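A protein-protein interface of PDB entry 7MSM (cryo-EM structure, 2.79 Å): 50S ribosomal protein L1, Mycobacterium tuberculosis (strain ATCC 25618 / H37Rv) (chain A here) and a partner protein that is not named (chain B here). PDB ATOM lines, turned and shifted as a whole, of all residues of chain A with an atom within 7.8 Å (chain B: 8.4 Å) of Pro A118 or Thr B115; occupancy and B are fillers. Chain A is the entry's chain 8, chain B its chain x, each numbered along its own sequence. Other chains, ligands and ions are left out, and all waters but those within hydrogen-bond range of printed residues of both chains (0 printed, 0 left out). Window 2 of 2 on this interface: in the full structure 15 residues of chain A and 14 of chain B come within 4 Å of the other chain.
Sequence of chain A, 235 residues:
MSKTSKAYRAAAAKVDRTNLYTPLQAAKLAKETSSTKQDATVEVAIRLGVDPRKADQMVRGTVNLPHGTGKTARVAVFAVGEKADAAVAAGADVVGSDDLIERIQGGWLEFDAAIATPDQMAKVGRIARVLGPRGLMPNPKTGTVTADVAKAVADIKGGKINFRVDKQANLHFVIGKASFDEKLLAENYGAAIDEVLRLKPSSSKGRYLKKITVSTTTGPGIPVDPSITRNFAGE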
ATOM      1  N   PHE A  78       7.396  -3.818   5.593  1.00  0.00           N
ATOM      2  CA  PHE A  78       6.895  -3.181   6.806  1.00  0.00           C
ATOM      3  C   PHE A  78       5.375  -3.282   6.840  1.00  0.00           C
ATOM      4  O   PHE A  78       4.683  -2.577   6.098  1.00  0.00           O
ATOM      5  CB  PHE A  78       7.350  -1.727   6.871  1.00  0.00           C
ATOM      6  CG  PHE A  78       8.830  -1.571   7.030  1.00  0.00           C
ATOM      7  CD1 PHE A  78       9.421  -1.691   8.278  1.00  0.00           C
ATOM      8  CD2 PHE A  78       9.634  -1.320   5.929  1.00  0.00           C
ATOM      9  CE1 PHE A  78      10.787  -1.554   8.428  1.00  0.00           C
ATOM     10  CE2 PHE A  78      10.999  -1.183   6.072  1.00  0.00           C
ATOM     11  CZ  PHE A  78      11.577  -1.299   7.323  1.00  0.00           C
ATOM     12  N   ALA A 116       6.392  -0.887   2.164  1.00  0.00           N
ATOM     13  CA  ALA A 116       5.528  -0.561   3.287  1.00  0.00           C
ATOM     14  C   ALA A 116       4.068  -0.512   2.851  1.00  0.00           C
ATOM     15  O   ALA A 116       3.728  -0.709   1.679  1.00  0.00           O
ATOM     16  CB  ALA A 116       5.956   0.765   3.920  1.00  0.00           C
ATOM     17  N   THR A 117       3.197  -0.244   3.827  1.00  0.00           N
ATOM     18  CA  THR A 117       1.755  -0.109   3.723  1.00  0.00           C
ATOM     19  C   THR A 117       1.340   1.332   4.014  1.00  0.00           C
ATOM     20  O   THR A 117       1.962   1.996   4.849  1.00  0.00           O
ATOM     21  CB  THR A 117       1.050  -1.051   4.708  1.00  0.00           C
ATOM     22  OG1 THR A 117       1.395  -0.682   6.049  1.00  0.00           O
ATOM     23  CG2 THR A 117       1.475  -2.487   4.461  1.00  0.00           C
ATOM     24  N   PRO A 118       0.298   1.847   3.347  1.00  0.00           N
ATOM     25  CA  PRO A 118      -0.029   3.277   3.487  1.00  0.00           C
ATOM     26  C   PRO A 118      -0.597   3.666   4.842  1.00  0.00           C
ATOM     27  O   PRO A 118      -0.614   4.861   5.160  1.00  0.00           O
ATOM     28  CB  PRO A 118      -1.061   3.511   2.374  1.00  0.00           C
ATOM     29  CG  PRO A 118      -0.846   2.399   1.409  1.00  0.00           C
ATOM     30  CD  PRO A 118      -0.470   1.226   2.255  1.00  0.00           C
ATOM     31  N   ASP A 119      -1.058   2.712   5.651  1.00  0.00           N
ATOM     32  CA  ASP A 119      -1.631   3.068   6.944  1.00  0.00           C
ATOM     33  C   ASP A 119      -0.557   3.319   7.997  1.00  0.00           C
ATOM     34  O   ASP A 119      -0.700   4.222   8.830  1.00  0.00           O
ATOM     35  CB  ASP A 119      -2.613   1.981   7.403  1.00  0.00           C
ATOM     36  CG  ASP A 119      -1.987   0.590   7.451  1.00  0.00           C
ATOM     37  OD1 ASP A 119      -0.818   0.425   7.043  1.00  0.00           O
ATOM     38  OD2 ASP A 119      -2.678  -0.349   7.900  1.00  0.00           O
ATOM     39  N   GLN A 120       0.524   2.542   7.970  1.00  0.00           N
ATOM     40  CA  GLN A 120       1.596   2.631   8.958  1.00  0.00           C
ATOM     41  C   GLN A 120       2.797   3.407   8.434  1.00  0.00           C
ATOM     42  O   GLN A 120       3.943   3.040   8.700  1.00  0.00           O
ATOM     43  CB  GLN A 120       2.016   1.236   9.412  1.00  0.00           C
ATOM     44  CG  GLN A 120       0.937   0.487  10.179  1.00  0.00           C
ATOM     45  CD  GLN A 120       0.613   1.133  11.516  1.00  0.00           C
ATOM     46  OE1 GLN A 120       1.502   1.617  12.217  1.00  0.00           O
ATOM     47  NE2 GLN A 120      -0.665   1.140  11.876  1.00  0.00           N
ATOM     48  N   MET A 121       2.567   4.475   7.671  1.00  0.00           N
ATOM     49  CA  MET A 121       3.660   5.297   7.167  1.00  0.00           C
ATOM     50  C   MET A 121       4.179   6.299   8.189  1.00  0.00           C
ATOM     51  O   MET A 121       5.103   7.054   7.869  1.00  0.00           O
ATOM     52  CB  MET A 121       3.222   6.051   5.911  1.00  0.00           C
ATOM     53  CG  MET A 121       2.917   5.167   4.719  1.00  0.00           C
ATOM     54  SD  MET A 121       4.322   4.184   4.163  1.00  0.00           S
ATOM     55  CE  MET A 121       5.383   5.452   3.475  1.00  0.00           C
ATOM     56  N   ALA A 122       3.601   6.339   9.393  1.00  0.00           N
ATOM     57  CA  ALA A 122       4.103   7.235  10.429  1.00  0.00           C
ATOM     58  C   ALA A 122       5.473   6.793  10.921  1.00  0.00           C
ATOM     59  O   ALA A 122       6.338   7.629  11.203  1.00  0.00           O
ATOM     60  CB  ALA A 122       3.112   7.302  11.589  1.00  0.00           C
ATOM     61  N   THR A 144       6.817   0.112  -4.216  1.00  0.00           N
ATOM     62  CA  THR A 144       7.076  -0.314  -2.847  1.00  0.00           C
ATOM     63  C   THR A 144       6.114   0.310  -1.847  1.00  0.00           C
ATOM     64  O   THR A 144       5.965  -0.216  -0.739  1.00  0.00           O
ATOM     65  CB  THR A 144       8.518   0.014  -2.457  1.00  0.00           C
ATOM     66  OG1 THR A 144       8.714   1.431  -2.492  1.00  0.00           O
ATOM     67  CG2 THR A 144       9.482  -0.639  -3.429  1.00  0.00           C
ATOM     68  N   VAL A 145       5.457   1.405  -2.204  1.00  0.00           N
ATOM     69  CA  VAL A 145       4.404   1.988  -1.383  1.00  0.00           C
ATOM     70  C   VAL A 145       3.090   1.668  -2.081  1.00  0.00           C
ATOM     71  O   VAL A 145       2.743   2.291  -3.090  1.00  0.00           O
ATOM     72  CB  VAL A 145       4.582   3.495  -1.189  1.00  0.00           C
ATOM     73  CG1 VAL A 145       3.474   4.043  -0.305  1.00  0.00           C
ATOM     74  CG2 VAL A 145       5.938   3.799  -0.608  1.00  0.00           C
ATOM     75  N   THR A 146       2.365   0.686  -1.553  1.00  0.00           N
ATOM     76  CA  THR A 146       1.087   0.280  -2.120  1.00  0.00           C
ATOM     77  C   THR A 146       0.270  -0.396  -1.030  1.00  0.00           C
ATOM     78  O   THR A 146       0.800  -0.798   0.009  1.00  0.00           O
ATOM     79  CB  THR A 146       1.269  -0.657  -3.322  1.00  0.00           C
ATOM     80  OG1 THR A 146      -0.005  -0.930  -3.917  1.00  0.00           O
ATOM     81  CG2 THR A 146       1.924  -1.962  -2.896  1.00  0.00           C
ATOM     82  N   ALA A 147      -1.035  -0.510  -1.285  1.00  0.00           N
ATOM     83  CA  ALA A 147      -1.929  -1.142  -0.319  1.00  0.00           C
ATOM     84  C   ALA A 147      -1.708  -2.649  -0.274  1.00  0.00           C
ATOM     85  O   ALA A 147      -1.336  -3.205   0.766  1.00  0.00           O
ATOM     86  CB  ALA A 147      -3.383  -0.814  -0.662  1.00  0.00           C
ATOM     87  N   ASP A 148      -1.924  -3.328  -1.397  1.00  0.00           N
ATOM     88  CA  ASP A 148      -1.713  -4.772  -1.482  1.00  0.00           C
ATOM     89  C   ASP A 148      -0.221  -5.028  -1.640  1.00  0.00           C
ATOM     90  O   ASP A 148       0.335  -4.889  -2.732  1.00  0.00           O
ATOM     91  CB  ASP A 148      -2.503  -5.367  -2.641  1.00  0.00           C
ATOM     92  CG  ASP A 148      -2.427  -6.881  -2.680  1.00  0.00           C
ATOM     93  OD1 ASP A 148      -3.086  -7.533  -1.844  1.00  0.00           O
ATOM     94  OD2 ASP A 148      -1.704  -7.419  -3.544  1.00  0.00           O
ATOM     95  N   VAL A 149       0.433  -5.419  -0.547  1.00  0.00           N
ATOM     96  CA  VAL A 149       1.878  -5.615  -0.543  1.00  0.00           C
ATOM     97  C   VAL A 149       2.212  -7.075  -0.814  1.00  0.00           C
ATOM     98  O   VAL A 149       3.351  -7.510  -0.617  1.00  0.00           O
ATOM     99  CB  VAL A 149       2.494  -5.147   0.788  1.00  0.00           C
ATOM    100  CG1 VAL A 149       2.262  -3.658   0.976  1.00  0.00           C
ATOM    101  CG2 VAL A 149       1.910  -5.932   1.954  1.00  0.00           C
ATOM    102  N   VAL B 106       3.287  15.185   6.721  1.00  0.00           N
ATOM    103  CA  VAL B 106       2.669  14.037   6.058  1.00  0.00           C
ATOM    104  C   VAL B 106       2.911  12.737   6.813  1.00  0.00           C
ATOM    105  O   VAL B 106       2.283  11.719   6.500  1.00  0.00           O
ATOM    106  CB  VAL B 106       3.192  13.951   4.608  1.00  0.00           C
ATOM    107  CG1 VAL B 106       4.574  13.321   4.560  1.00  0.00           C
ATOM    108  CG2 VAL B 106       2.202  13.257   3.669  1.00  0.00           C
ATOM    109  N   ALA B 107       3.793  12.741   7.813  1.00  0.00           N
ATOM    110  CA  ALA B 107       3.977  11.553   8.636  1.00  0.00           C
ATOM    111  C   ALA B 107       2.791  11.298   9.559  1.00  0.00           C
ATOM    112  O   ALA B 107       2.573  10.151   9.961  1.00  0.00           O
ATOM    113  CB  ALA B 107       5.261  11.671   9.457  1.00  0.00           C
ATOM    114  N   LEU B 109      -0.471  13.581   9.269  1.00  0.00           N
ATOM    115  CA  LEU B 109      -1.733  14.032   8.691  1.00  0.00           C
ATOM    116  C   LEU B 109      -2.242  13.058   7.636  1.00  0.00           C
ATOM    117  O   LEU B 109      -3.454  12.967   7.413  1.00  0.00           O
ATOM    118  CB  LEU B 109      -1.564  15.440   8.109  1.00  0.00           C
ATOM    119  CG  LEU B 109      -2.765  16.271   7.641  1.00  0.00           C
ATOM    120  CD1 LEU B 109      -2.497  17.738   7.929  1.00  0.00           C
ATOM    121  CD2 LEU B 109      -3.052  16.096   6.151  1.00  0.00           C
ATOM    122  N   MET B 110      -1.341  12.324   6.988  1.00  0.00           N
ATOM    123  CA  MET B 110      -1.756  11.367   5.970  1.00  0.00           C
ATOM    124  C   MET B 110      -2.281  10.078   6.590  1.00  0.00           C
ATOM    125  O   MET B 110      -3.104   9.391   5.974  1.00  0.00           O
ATOM    126  CB  MET B 110      -0.581  11.108   5.015  1.00  0.00           C
ATOM    127  CG  MET B 110      -0.849  10.207   3.821  1.00  0.00           C
ATOM    128  SD  MET B 110      -0.433   8.482   4.113  1.00  0.00           S
ATOM    129  CE  MET B 110       1.348   8.587   3.996  1.00  0.00           C
ATOM    130  N   ALA B 111      -1.867   9.764   7.823  1.00  0.00           N
ATOM    131  CA  ALA B 111      -2.229   8.495   8.448  1.00  0.00           C
ATOM    132  C   ALA B 111      -3.704   8.414   8.832  1.00  0.00           C
ATOM    133  O   ALA B 111      -4.219   7.306   9.016  1.00  0.00           O
ATOM    134  CB  ALA B 111      -1.359   8.254   9.682  1.00  0.00           C
ATOM    135  N   THR B 112      -4.394   9.548   8.952  1.00  0.00           N
ATOM    136  CA  THR B 112      -5.817   9.546   9.256  1.00  0.00           C
ATOM    137  C   THR B 112      -6.689   9.977   8.085  1.00  0.00           C
ATOM    138  O   THR B 112      -7.908   9.783   8.142  1.00  0.00           O
ATOM    139  CB  THR B 112      -6.108  10.450  10.466  1.00  0.00           C
ATOM    140  OG1 THR B 112      -7.487  10.323  10.839  1.00  0.00           O
ATOM    141  CG2 THR B 112      -5.805  11.905  10.142  1.00  0.00           C
ATOM    142  N   ASP B 113      -6.108  10.547   7.035  1.00  0.00           N
ATOM    143  CA  ASP B 113      -6.841  10.974   5.855  1.00  0.00           C
ATOM    144  C   ASP B 113      -6.752   9.910   4.766  1.00  0.00           C
ATOM    145  O   ASP B 113      -6.330   8.774   5.005  1.00  0.00           O
ATOM    146  CB  ASP B 113      -6.323  12.329   5.373  1.00  0.00           C
ATOM    147  CG  ASP B 113      -6.728  13.463   6.288  1.00  0.00           C
ATOM    148  OD1 ASP B 113      -7.791  13.351   6.935  1.00  0.00           O
ATOM    149  OD2 ASP B 113      -5.990  14.466   6.359  1.00  0.00           O
ATOM    150  N   TYR B 114      -7.174  10.277   3.556  1.00  0.00           N
ATOM    151  CA  TYR B 114      -7.161   9.362   2.420  1.00  0.00           C
ATOM    152  C   TYR B 114      -5.726   9.062   1.996  1.00  0.00           C
ATOM    153  O   TYR B 114      -4.946   9.974   1.706  1.00  0.00           O
ATOM    154  CB  TYR B 114      -7.989   9.936   1.265  1.00  0.00           C
ATOM    155  CG  TYR B 114      -7.591  11.313   0.754  1.00  0.00           C
ATOM    156  CD1 TYR B 114      -8.093  12.470   1.348  1.00  0.00           C
ATOM    157  CD2 TYR B 114      -6.765  11.456  -0.357  1.00  0.00           C
ATOM    158  CE1 TYR B 114      -7.746  13.726   0.877  1.00  0.00           C
ATOM    159  CE2 TYR B 114      -6.411  12.706  -0.832  1.00  0.00           C
ATOM    160  CZ  TYR B 114      -6.906  13.836  -0.214  1.00  0.00           C
ATOM    161  OH  TYR B 114      -6.558  15.079  -0.690  1.00  0.00           O
ATOM    162  N   THR B 115      -5.362   7.788   2.034  1.00  0.00           N
ATOM    163  CA  THR B 115      -4.005   7.347   1.711  1.00  0.00           C
ATOM    164  C   THR B 115      -3.889   6.874   0.266  1.00  0.00           C
ATOM    165  O   THR B 115      -3.372   5.787   0.008  1.00  0.00           O
ATOM    166  CB  THR B 115      -3.582   6.246   2.675  1.00  0.00           C
ATOM    167  OG1 THR B 115      -4.423   5.101   2.483  1.00  0.00           O
ATOM    168  CG2 THR B 115      -3.720   6.716   4.111  1.00  0.00           C
ATOM    169  N   ASP B 116      -4.355   7.661  -0.697  1.00  0.00           N
ATOM    170  CA  ASP B 116      -4.127   7.267  -2.086  1.00  0.00           C
ATOM    171  C   ASP B 116      -3.557   8.383  -2.952  1.00  0.00           C
ATOM    172  O   ASP B 116      -2.700   8.116  -3.798  1.00  0.00           O
ATOM    173  CB  ASP B 116      -5.427   6.714  -2.714  1.00  0.00           C
ATOM    174  CG  ASP B 116      -6.584   7.697  -2.659  1.00  0.00           C
ATOM    175  OD1 ASP B 116      -6.450   8.771  -2.039  1.00  0.00           O
ATOM    176  OD2 ASP B 116      -7.641   7.390  -3.251  1.00  0.00           O
ATOM    177  N   GLU B 117      -4.006   9.625  -2.761  1.00  0.00           N
ATOM    178  CA  GLU B 117      -3.483  10.743  -3.537  1.00  0.00           C
ATOM    179  C   GLU B 117      -2.307  11.408  -2.841  1.00  0.00           C
ATOM    180  O   GLU B 117      -1.430  11.968  -3.510  1.00  0.00           O
ATOM    181  CB  GLU B 117      -4.598  11.763  -3.805  1.00  0.00           C
ATOM    182  CG  GLU B 117      -4.304  12.800  -4.893  1.00  0.00           C
ATOM    183  CD  GLU B 117      -3.613  14.048  -4.368  1.00  0.00           C
ATOM    184  OE1 GLU B 117      -3.814  14.382  -3.181  1.00  0.00           O
ATOM    185  OE2 GLU B 117      -2.872  14.691  -5.140  1.00  0.00           O
ATOM    186  N   LEU B 118      -2.252  11.327  -1.514  1.00  0.00           N
ATOM    187  CA  LEU B 118      -1.116  11.822  -0.750  1.00  0.00           C
ATOM    188  C   LEU B 118       0.084  10.888  -0.813  1.00  0.00           C
ATOM    189  O   LEU B 118       1.133  11.214  -0.249  1.00  0.00           O
ATOM    190  CB  LEU B 118      -1.525  12.040   0.708  1.00  0.00           C
ATOM    191  CG  LEU B 118      -2.628  13.066   0.969  1.00  0.00           C
ATOM    192  CD1 LEU B 118      -3.000  13.087   2.442  1.00  0.00           C
ATOM    193  CD2 LEU B 118      -2.211  14.446   0.494  1.00  0.00           C
ATOM    194  N   MET B 119      -0.057   9.732  -1.468  1.00  0.00           N
ATOM    195  CA  MET B 119       1.062   8.818  -1.667  1.00  0.00           C
ATOM    196  C   MET B 119       2.131   9.433  -2.559  1.00  0.00           C
ATOM    197  O   MET B 119       3.330   9.257  -2.314  1.00  0.00           O
ATOM    198  CB  MET B 119       0.545   7.510  -2.264  1.00  0.00           C
ATOM    199  CG  MET B 119       1.584   6.430  -2.438  1.00  0.00           C
ATOM    200  SD  MET B 119       0.857   4.940  -3.144  1.00  0.00           S
ATOM    201  CE  MET B 119      -0.098   4.335  -1.756  1.00  0.00           C
ATOM    202  N   GLU B 120       1.719  10.160  -3.596  1.00  0.00           N
ATOM    203  CA  GLU B 120       2.666  10.876  -4.437  1.00  0.00           C
ATOM    204  C   GLU B 120       2.980  12.273  -3.916  1.00  0.00           C
ATOM    205  O   GLU B 120       3.998  12.850  -4.311  1.00  0.00           O
ATOM    206  CB  GLU B 120       2.141  10.945  -5.878  1.00  0.00           C
ATOM    207  CG  GLU B 120       0.765  11.583  -6.049  1.00  0.00           C
ATOM    208  CD  GLU B 120       0.825  13.076  -6.303  1.00  0.00           C
ATOM    209  OE1 GLU B 120       1.899  13.571  -6.703  1.00  0.00           O
ATOM    210  OE2 GLU B 120      -0.206  13.751  -6.108  1.00  0.00           O
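Hydrophobic or aromatic side chains of chain A within 4 Å of the printed part of chain B: Pro A118, Met A121, Ala A122 and Val A145. Printed residues of chain B that touch a printed residue of chain A: Ala B107, Met B110, Thr B115 and Met B119. Hydrophobic or aromatic side chains of chain B that line the printed part of chain A: Met B110 and Met B119. Among the printed residues, 6 pairs touch across the chains.
O of Pro A118 sits close to SD of Met B110 (3.8 Å). The backbone carbonyl oxygen (O) of Val A145 lies close to the side-chain sulfur (SD) of Met B119 (3.3 Å).
Of the printed residues of chain B, Pro A118 touches Met B110 (3.8 Å), Thr B115 (3.7 Å) and Met B119 (3.8 Å). Thr B115 touches one residue of chain A. Of the printed residues of chain A, Ala B107 touches Ala A122 (3.3 Å). Of the printed residues of chain B, Val A145 touches Met B119 (3.3 Å). Printed residues of chain A within 4 Å of Met B110: Pro A118 (3.8 Å) and Met A121 (3.7 Å). Thr A144 touches none of the printed residues of chain B. The nearest printed residue of chain B that does not touch Ala A122 is Ala B111 (5.0 Å).
CB of Pro A118 touches OG1 of Thr B115, at 3.7 Å. CG of Pro A118 touches CE of Met B119, at 3.8 Å. Met A121 touches Met B110 (CB to CE, 3.7 Å). O of Ala B107 touches CB of Ala A122, 3.3 Å away.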
